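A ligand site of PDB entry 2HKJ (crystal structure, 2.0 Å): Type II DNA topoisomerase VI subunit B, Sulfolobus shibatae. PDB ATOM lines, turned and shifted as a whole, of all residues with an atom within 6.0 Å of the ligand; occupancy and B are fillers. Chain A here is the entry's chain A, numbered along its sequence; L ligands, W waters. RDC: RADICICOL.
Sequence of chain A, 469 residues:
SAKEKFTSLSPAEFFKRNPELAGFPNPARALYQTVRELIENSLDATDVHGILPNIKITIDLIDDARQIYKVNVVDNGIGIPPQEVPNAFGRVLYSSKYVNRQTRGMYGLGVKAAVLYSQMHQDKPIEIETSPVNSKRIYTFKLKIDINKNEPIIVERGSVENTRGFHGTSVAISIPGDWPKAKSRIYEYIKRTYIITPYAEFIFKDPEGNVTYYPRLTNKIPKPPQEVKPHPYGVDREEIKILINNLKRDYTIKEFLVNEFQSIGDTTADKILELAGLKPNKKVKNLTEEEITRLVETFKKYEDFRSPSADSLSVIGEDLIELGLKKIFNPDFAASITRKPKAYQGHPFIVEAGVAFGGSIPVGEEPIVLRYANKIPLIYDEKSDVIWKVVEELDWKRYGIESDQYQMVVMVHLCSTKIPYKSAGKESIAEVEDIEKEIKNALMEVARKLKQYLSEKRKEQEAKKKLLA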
ATOM      1  N   GLU A  37      -1.190  18.693 -19.123  1.00  0.00           N
ATOM      2  CA  GLU A  37      -2.075  18.087 -20.143  1.00  0.00           C
ATOM      3  C   GLU A  37      -3.535  18.409 -19.844  1.00  0.00           C
ATOM      4  O   GLU A  37      -4.299  18.735 -20.765  1.00  0.00           O
ATOM      5  CB  GLU A  37      -1.912  16.556 -20.196  1.00  0.00           C
ATOM      6  CG  GLU A  37      -0.489  16.033 -20.604  1.00  0.00           C
ATOM      7  CD  GLU A  37      -0.007  16.554 -21.951  1.00  0.00           C
ATOM      8  OE1 GLU A  37       1.232  16.584 -22.194  1.00  0.00           O
ATOM      9  OE2 GLU A  37      -0.867  16.911 -22.790  1.00  0.00           O
ATOM     10  N   LEU A  38      -3.952  18.303 -18.581  1.00  0.00           N
ATOM     11  CA  LEU A  38      -5.364  18.600 -18.268  1.00  0.00           C
ATOM     12  C   LEU A  38      -5.717  20.079 -18.471  1.00  0.00           C
ATOM     13  O   LEU A  38      -6.785  20.400 -19.041  1.00  0.00           O
ATOM     14  CB  LEU A  38      -5.718  18.129 -16.865  1.00  0.00           C
ATOM     15  CG  LEU A  38      -5.568  16.616 -16.655  1.00  0.00           C
ATOM     16  CD1 LEU A  38      -5.846  16.281 -15.171  1.00  0.00           C
ATOM     17  CD2 LEU A  38      -6.483  15.778 -17.626  1.00  0.00           C
ATOM     18  N   ILE A  39      -4.841  20.986 -18.007  1.00  0.00           N
ATOM     19  CA  ILE A  39      -5.098  22.420 -18.195  1.00  0.00           C
ATOM     20  C   ILE A  39      -5.135  22.796 -19.685  1.00  0.00           C
ATOM     21  O   ILE A  39      -6.058  23.519 -20.140  1.00  0.00           O
ATOM     22  CB  ILE A  39      -4.115  23.275 -17.405  1.00  0.00           C
ATOM     23  CG1 ILE A  39      -4.412  23.183 -15.888  1.00  0.00           C
ATOM     24  CG2 ILE A  39      -4.173  24.778 -17.884  1.00  0.00           C
ATOM     25  CD1 ILE A  39      -3.280  23.919 -15.032  1.00  0.00           C
ATOM     26  N   GLU A  40      -4.173  22.286 -20.435  1.00  0.00           N
ATOM     27  CA  GLU A  40      -4.122  22.540 -21.884  1.00  0.00           C
ATOM     28  C   GLU A  40      -5.360  22.076 -22.658  1.00  0.00           C
ATOM     29  O   GLU A  40      -5.924  22.840 -23.477  1.00  0.00           O
ATOM     30  CB  GLU A  40      -2.794  22.045 -22.465  1.00  0.00           C
ATOM     31  CG  GLU A  40      -1.650  22.906 -21.952  1.00  0.00           C
ATOM     32  CD  GLU A  40      -0.271  22.252 -22.095  1.00  0.00           C
ATOM     33  OE1 GLU A  40      -0.109  21.345 -22.943  1.00  0.00           O
ATOM     34  OE2 GLU A  40       0.654  22.689 -21.375  1.00  0.00           O
ATOM     35  N   ASN A  41      -5.832  20.851 -22.352  1.00  0.00           N
ATOM     36  CA  ASN A  41      -7.058  20.321 -22.971  1.00  0.00           C
ATOM     37  C   ASN A  41      -8.286  21.181 -22.580  1.00  0.00           C
ATOM     38  O   ASN A  41      -9.129  21.502 -23.431  1.00  0.00           O
ATOM     39  CB  ASN A  41      -7.271  18.864 -22.524  1.00  0.00           C
ATOM     40  CG  ASN A  41      -6.415  17.896 -23.311  1.00  0.00           C
ATOM     41  OD1 ASN A  41      -5.719  18.280 -24.259  1.00  0.00           O
ATOM     42  ND2 ASN A  41      -6.472  16.602 -22.938  1.00  0.00           N
ATOM     43  N   SER A  42      -8.340  21.581 -21.311  1.00  0.00           N
ATOM     44  CA  SER A  42      -9.451  22.423 -20.808  1.00  0.00           C
ATOM     45  C   SER A  42      -9.500  23.778 -21.495  1.00  0.00           C
ATOM     46  O   SER A  42     -10.608  24.318 -21.757  1.00  0.00           O
ATOM     47  CB  SER A  42      -9.378  22.570 -19.266  1.00  0.00           C
ATOM     48  OG  SER A  42      -9.763  21.319 -18.659  1.00  0.00           O
ATOM     49  N   ASP A  44      -8.201  24.330 -24.600  1.00  0.00           N
ATOM     50  CA  ASP A  44      -8.538  24.079 -26.019  1.00  0.00           C
ATOM     51  C   ASP A  44     -10.045  23.768 -26.142  1.00  0.00           C
ATOM     52  O   ASP A  44     -10.637  23.930 -27.226  1.00  0.00           O
ATOM     53  CB  ASP A  44      -7.677  22.900 -26.577  1.00  0.00           C
ATOM     54  CG  ASP A  44      -6.292  23.360 -27.111  1.00  0.00           C
ATOM     55  OD1 ASP A  44      -6.036  24.587 -27.106  1.00  0.00           O
ATOM     56  OD2 ASP A  44      -5.482  22.506 -27.560  1.00  0.00           O
ATOM     57  N   ALA A  45     -10.647  23.298 -25.041  1.00  0.00           N
ATOM     58  CA  ALA A  45     -12.085  22.956 -25.021  1.00  0.00           C
ATOM     59  C   ALA A  45     -12.985  24.144 -24.817  1.00  0.00           C
ATOM     60  O   ALA A  45     -14.215  24.054 -25.031  1.00  0.00           O
ATOM     61  CB  ALA A  45     -12.405  21.910 -23.941  1.00  0.00           C
ATOM     62  N   THR A  46     -12.369  25.260 -24.410  1.00  0.00           N
ATOM     63  CA  THR A  46     -13.092  26.485 -24.060  1.00  0.00           C
ATOM     64  C   THR A  46     -12.827  27.606 -25.056  1.00  0.00           C
ATOM     65  O   THR A  46     -13.689  27.916 -25.863  1.00  0.00           O
ATOM     66  CB  THR A  46     -12.773  26.966 -22.606  1.00  0.00           C
ATOM     67  OG1 THR A  46     -11.364  26.816 -22.340  1.00  0.00           O
ATOM     68  CG2 THR A  46     -13.532  26.125 -21.573  1.00  0.00           C
ATOM     69  N   HIS A  49     -13.421  27.637 -28.712  1.00  0.00           N
ATOM     70  CA  HIS A  49     -14.848  27.566 -29.075  1.00  0.00           C
ATOM     71  C   HIS A  49     -15.664  28.735 -28.583  1.00  0.00           C
ATOM     72  O   HIS A  49     -16.890  28.651 -28.493  1.00  0.00           O
ATOM     73  CB  HIS A  49     -15.416  26.226 -28.553  1.00  0.00           C
ATOM     74  CG  HIS A  49     -14.687  25.051 -29.101  1.00  0.00           C
ATOM     75  ND1 HIS A  49     -14.904  24.558 -30.375  1.00  0.00           N
ATOM     76  CD2 HIS A  49     -13.648  24.334 -28.601  1.00  0.00           C
ATOM     77  CE1 HIS A  49     -14.053  23.578 -30.622  1.00  0.00           C
ATOM     78  NE2 HIS A  49     -13.293  23.411 -29.551  1.00  0.00           N
ATOM     79  N   VAL A  73      -9.081  18.140 -12.829  1.00  0.00           N
ATOM     80  CA  VAL A  73      -9.328  19.402 -13.546  1.00  0.00           C
ATOM     81  C   VAL A  73     -10.737  19.438 -14.096  1.00  0.00           C
ATOM     82  O   VAL A  73     -11.200  18.442 -14.676  1.00  0.00           O
ATOM     83  CB  VAL A  73      -8.321  19.616 -14.700  1.00  0.00           C
ATOM     84  CG1 VAL A  73      -8.675  20.942 -15.476  1.00  0.00           C
ATOM     85  CG2 VAL A  73      -6.898  19.704 -14.107  1.00  0.00           C
ATOM     86  N   ASP A  75     -13.598  21.877 -16.238  1.00  0.00           N
ATOM     87  CA  ASP A  75     -13.768  23.001 -17.118  1.00  0.00           C
ATOM     88  C   ASP A  75     -15.233  23.186 -17.565  1.00  0.00           C
ATOM     89  O   ASP A  75     -16.076  22.291 -17.363  1.00  0.00           O
ATOM     90  CB  ASP A  75     -12.805  22.886 -18.309  1.00  0.00           C
ATOM     91  CG  ASP A  75     -13.157  21.705 -19.238  1.00  0.00           C
ATOM     92  OD1 ASP A  75     -12.272  20.840 -19.472  1.00  0.00           O
ATOM     93  OD2 ASP A  75     -14.325  21.653 -19.725  1.00  0.00           O
ATOM     94  N   GLY A  77     -16.003  23.706 -20.843  1.00  0.00           N
ATOM     95  CA  GLY A  77     -15.818  23.709 -22.280  1.00  0.00           C
ATOM     96  C   GLY A  77     -16.953  23.003 -23.002  1.00  0.00           C
ATOM     97  O   GLY A  77     -18.055  22.822 -22.437  1.00  0.00           O
ATOM     98  N   ILE A  78     -16.680  22.597 -24.237  1.00  0.00           N
ATOM     99  CA  ILE A  78     -17.727  22.034 -25.091  1.00  0.00           C
ATOM    100  C   ILE A  78     -18.075  20.570 -24.805  1.00  0.00           C
ATOM    101  O   ILE A  78     -19.008  20.033 -25.414  1.00  0.00           O
ATOM    102  CB  ILE A  78     -17.380  22.205 -26.607  1.00  0.00           C
ATOM    103  CG1 ILE A  78     -16.083  21.497 -26.979  1.00  0.00           C
ATOM    104  CG2 ILE A  78     -17.282  23.688 -26.941  1.00  0.00           C
ATOM    105  CD1 ILE A  78     -15.926  21.280 -28.504  1.00  0.00           C
ATOM    106  N   GLY A  79     -17.342  19.915 -23.906  1.00  0.00           N
ATOM    107  CA  GLY A  79     -17.614  18.514 -23.559  1.00  0.00           C
ATOM    108  C   GLY A  79     -17.193  17.494 -24.613  1.00  0.00           C
ATOM    109  O   GLY A  79     -16.726  17.863 -25.691  1.00  0.00           O
ATOM    110  N   ILE A  80     -17.326  16.215 -24.294  1.00  0.00           N
ATOM    111  CA  ILE A  80     -16.908  15.121 -25.177  1.00  0.00           C
ATOM    112  C   ILE A  80     -18.113  14.246 -25.460  1.00  0.00           C
ATOM    113  O   ILE A  80     -18.783  13.804 -24.544  1.00  0.00           O
ATOM    114  CB  ILE A  80     -15.838  14.167 -24.535  1.00  0.00           C
ATOM    115  CG1 ILE A  80     -14.805  14.940 -23.728  1.00  0.00           C
ATOM    116  CG2 ILE A  80     -15.162  13.293 -25.627  1.00  0.00           C
ATOM    117  CD1 ILE A  80     -14.073  14.067 -22.714  1.00  0.00           C
ATOM    118  N   PRO A  81     -18.394  13.999 -26.741  1.00  0.00           N
ATOM    119  CA  PRO A  81     -19.489  13.113 -27.027  1.00  0.00           C
ATOM    120  C   PRO A  81     -19.214  11.765 -26.340  1.00  0.00           C
ATOM    121  O   PRO A  81     -18.102  11.237 -26.405  1.00  0.00           O
ATOM    122  CB  PRO A  81     -19.441  13.013 -28.560  1.00  0.00           C
ATOM    123  CG  PRO A  81     -18.856  14.375 -28.979  1.00  0.00           C
ATOM    124  CD  PRO A  81     -17.748  14.505 -27.964  1.00  0.00           C
ATOM    125  N   GLU A  84     -17.192   8.927 -27.836  1.00  0.00           N
ATOM    126  CA  GLU A  84     -15.780   9.172 -28.106  1.00  0.00           C
ATOM    127  C   GLU A  84     -14.880   9.051 -26.857  1.00  0.00           C
ATOM    128  O   GLU A  84     -13.636   9.005 -26.963  1.00  0.00           O
ATOM    129  CB  GLU A  84     -15.631  10.543 -28.730  1.00  0.00           C
ATOM    130  CG  GLU A  84     -16.061  10.576 -30.213  1.00  0.00           C
ATOM    131  CD  GLU A  84     -16.278  11.980 -30.729  1.00  0.00           C
ATOM    132  OE1 GLU A  84     -15.531  12.894 -30.326  1.00  0.00           O
ATOM    133  OE2 GLU A  84     -17.199  12.180 -31.566  1.00  0.00           O
ATOM    134  N   ALA A  88     -10.696   8.362 -26.440  1.00  0.00           N
ATOM    135  CA  ALA A  88     -10.002   9.615 -26.142  1.00  0.00           C
ATOM    136  C   ALA A  88      -8.951   9.417 -25.018  1.00  0.00           C
ATOM    137  O   ALA A  88      -7.911  10.077 -25.011  1.00  0.00           O
ATOM    138  CB  ALA A  88     -11.013  10.679 -25.748  1.00  0.00           C
ATOM    139  N   PHE A  89      -9.263   8.549 -24.044  1.00  0.00           N
ATOM    140  CA  PHE A  89      -8.410   8.314 -22.875  1.00  0.00           C
ATOM    141  C   PHE A  89      -7.647   6.976 -22.930  1.00  0.00           C
ATOM    142  O   PHE A  89      -6.583   6.829 -22.305  1.00  0.00           O
ATOM    143  CB  PHE A  89      -9.233   8.377 -21.576  1.00  0.00           C
ATOM    144  CG  PHE A  89      -9.827   9.742 -21.299  1.00  0.00           C
ATOM    145  CD1 PHE A  89      -9.135  10.686 -20.542  1.00  0.00           C
ATOM    146  CD2 PHE A  89     -11.080  10.091 -21.803  1.00  0.00           C
ATOM    147  CE1 PHE A  89      -9.653  11.978 -20.326  1.00  0.00           C
ATOM    148  CE2 PHE A  89     -11.619  11.370 -21.567  1.00  0.00           C
ATOM    149  CZ  PHE A  89     -10.902  12.301 -20.803  1.00  0.00           C
ATOM    150  N   VAL A 111      -3.153  13.669 -22.950  1.00  0.00           N
ATOM    151  CA  VAL A 111      -3.639  13.070 -21.713  1.00  0.00           C
ATOM    152  C   VAL A 111      -3.401  11.548 -21.659  1.00  0.00           C
ATOM    153  O   VAL A 111      -3.283  10.975 -20.584  1.00  0.00           O
ATOM    154  CB  VAL A 111      -5.157  13.369 -21.521  1.00  0.00           C
ATOM    155  CG1 VAL A 111      -6.037  12.554 -22.485  1.00  0.00           C
ATOM    156  CG2 VAL A 111      -5.610  13.146 -20.080  1.00  0.00           C
ATOM    157  N   THR A 130     -18.680  14.263 -18.289  1.00  0.00           N
ATOM    158  CA  THR A 130     -18.736  15.220 -19.375  1.00  0.00           C
ATOM    159  C   THR A 130     -20.174  15.511 -19.829  1.00  0.00           C
ATOM    160  O   THR A 130     -21.021  14.614 -19.865  1.00  0.00           O
ATOM    161  CB  THR A 130     -17.860  14.769 -20.577  1.00  0.00           C
ATOM    162  OG1 THR A 130     -17.776  15.824 -21.528  1.00  0.00           O
ATOM    163  CG2 THR A 130     -18.411  13.493 -21.267  1.00  0.00           C
ATOM    164  N   GLY A 168     -19.412  20.805 -20.173  1.00  0.00           N
ATOM    165  CA  GLY A 168     -17.982  20.805 -19.900  1.00  0.00           C
ATOM    166  C   GLY A 168     -17.539  19.414 -19.492  1.00  0.00           C
ATOM    167  O   GLY A 168     -18.286  18.437 -19.689  1.00  0.00           O
ATOM    168  N   THR A 169     -16.353  19.344 -18.915  1.00  0.00           N
ATOM    169  CA  THR A 169     -15.706  18.084 -18.633  1.00  0.00           C
ATOM    170  C   THR A 169     -14.908  18.147 -17.337  1.00  0.00           C
ATOM    171  O   THR A 169     -14.222  19.165 -17.049  1.00  0.00           O
ATOM    172  CB  THR A 169     -14.741  17.697 -19.759  1.00  0.00           C
ATOM    173  OG1 THR A 169     -15.482  17.534 -20.976  1.00  0.00           O
ATOM    174  CG2 THR A 169     -13.967  16.400 -19.439  1.00  0.00           C
ATOM    175  N   VAL A 171     -12.043  15.683 -15.263  1.00  0.00           N
ATOM    176  CA  VAL A 171     -11.146  14.543 -15.387  1.00  0.00           C
ATOM    177  C   VAL A 171     -10.384  14.443 -14.071  1.00  0.00           C
ATOM    178  O   VAL A 171      -9.904  15.458 -13.547  1.00  0.00           O
ATOM    179  CB  VAL A 171     -10.102  14.702 -16.541  1.00  0.00           C
ATOM    180  CG1 VAL A 171      -9.116  13.508 -16.552  1.00  0.00           C
ATOM    181  CG2 VAL A 171     -10.746  14.877 -17.930  1.00  0.00           C
HETATM  182  C1  RDC L   1     -12.861  17.800 -23.832  1.00  0.00           C
HETATM  183  C2  RDC L   1     -11.822  17.537 -22.826  1.00  0.00           C
HETATM  184  C3  RDC L   1     -11.590  18.533 -21.760  1.00  0.00           C
HETATM  185  C4  RDC L   1     -10.627  18.322 -20.799  1.00  0.00           C
HETATM  186  C5  RDC L   1      -9.800  17.197 -20.875  1.00  0.00           C
HETATM  187  C6  RDC L   1      -9.956  16.225 -21.931  1.00  0.00           C
HETATM  188  C7  RDC L   1     -10.971  16.338 -22.958  1.00  0.00           C
HETATM  189  C8  RDC L   1     -11.124  15.253 -24.006  1.00  0.00           C
HETATM  190  C9  RDC L   1      -9.834  14.894 -24.754  1.00  0.00           C
HETATM  191  C10 RDC L   1      -9.025  15.868 -25.522  1.00  0.00           C
HETATM  192  C11 RDC L   1      -9.289  17.179 -25.533  1.00  0.00           C
HETATM  193  C12 RDC L   1      -8.483  18.080 -26.345  1.00  0.00           C
HETATM  194  C13 RDC L   1      -8.953  19.289 -26.712  1.00  0.00           C
HETATM  195  C14 RDC L   1     -10.335  19.749 -26.308  1.00  0.00           C
HETATM  196  C15 RDC L   1     -11.425  19.426 -27.348  1.00  0.00           C
HETATM  197  C16 RDC L   1     -12.823  19.464 -26.689  1.00  0.00           C
HETATM  198  C17 RDC L   1     -13.319  18.127 -26.150  1.00  0.00           C
HETATM  199  C18 RDC L   1     -13.344  16.991 -27.159  1.00  0.00           C
HETATM  200  O1  RDC L   1     -12.389  17.683 -25.164  1.00  0.00           O
HETATM  201  O2  RDC L   1     -13.996  18.134 -23.582  1.00  0.00           O
HETATM  202  O3  RDC L   1     -12.404  19.602 -21.688  1.00  0.00           O
HETATM  203  O4  RDC L   1      -8.788  16.974 -19.997  1.00  0.00           O
HETATM  204 CL1  RDC L   1      -8.942  14.776 -21.943  1.00  0.00          CL
HETATM  205  O5  RDC L   1      -9.475  13.719 -24.759  1.00  0.00           O
HETATM  206  O6  RDC L   1     -10.843  20.720 -27.222  1.00  0.00           O
HETATM  207  O   HOH W   1      -6.836  20.488 -28.809  1.00  0.00           O
HETATM  208  O   HOH W   2     -10.771  22.347 -29.516  1.00  0.00           O
HETATM  209  O   HOH W   3     -15.036  20.350 -22.039  1.00  0.00           O
HETATM  210  O   HOH W   4      -7.395  12.580 -26.013  1.00  0.00           O
HETATM  211  O   HOH W   5     -11.429  18.600 -17.475  1.00  0.00           O
HETATM  212  O   HOH W   6      -8.825  18.643 -18.246  1.00  0.00           O
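The backbone NH (N) of Asp 75 sits at hydrogen-bond distance from the backbone carbonyl oxygen (O) of Thr 169 (2.9 Å). The side-chain carboxylate of Asp 75 sits at hydrogen-bond distance from the side-chain hydroxyl of Ser 42, 2.7 Å away. The backbone NH of Gly 77 lies within hydrogen-bond range of the side-chain carboxylate of Asp 75, at 2.9 Å. The side-chain hydroxyl (OG1) of Thr 130 sits at hydrogen-bond distance from the side-chain hydroxyl (OG1) of Thr 169 (2.9 Å). The backbone carbonyl oxygen of Ala 45 is in hydrogen-bond range of the backbone NH of Ile 78 (3.0 Å). The backbone NH (N) of Ile 80 sits at hydrogen-bond distance from the side-chain hydroxyl (OG1) of Thr 130 (2.8 Å). O of Leu 38 sits at hydrogen-bond distance from OG of Ser 42 (3.1 Å). The backbone NH (N) of Val 73 lies within hydrogen-bond range of the backbone carbonyl oxygen (O) of Val 171 (2.9 Å).
OD1 of Asp 75 lies within hydrogen-bond range of O3 of the ligand, at 2.5 Å. An oxygen (O2) of the ligand lies within hydrogen-bond range of the side-chain hydroxyl of Thr 169, 3.1 Å away. An oxygen (O6) of the ligand sits close to the backbone NH (N) of Ala 45.
Water W6 lies within hydrogen-bond range of O4 of the ligand (2.4 Å), O of Leu 38 (2.8 Å) and OG of Ser 42 (2.9 Å). Water W4 bridges O5 of the ligand (2.7 Å) and O of Ala 88 (2.7 Å). Water W3 lies within hydrogen-bond range of the side-chain carboxylate of Asp 75, an oxygen (O3) of the ligand, the backbone NH of Gly 79 and the side-chain hydroxyl of Thr 169. Water W2 lies within hydrogen-bond range of a ring nitrogen (NE2) of His 49 (2.7 Å), the backbone carbonyl oxygen (O) of Asp 44 (2.8 Å) and an oxygen (O6) of the ligand (2.8 Å).
O of Asp 44 sits close to O6 of the ligand. O of Gly 79 lies close to O2 of the ligand (3.5 Å). Merely in contact with the ligand: Leu 38 (3.5 Å), Asn 41 (3.2 Å), Ser 42 (3.8 Å), Ile 78 (3.9 Å), Ile 80 (3.3 Å), Ala 88 (3.5 Å), Phe 89 (3.3 Å), Val 111 (3.7 Å) and Val 171 (3.5 Å). Hydrophobic or aromatic side chains within 4 Å of the ligand: Leu 38, Ala 45, Ile 78, Ile 80, Ala 88, Phe 89, Val 111 and Val 171. The nearest printed residue that does not touch the ligand is His 49 (4.3 Å).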
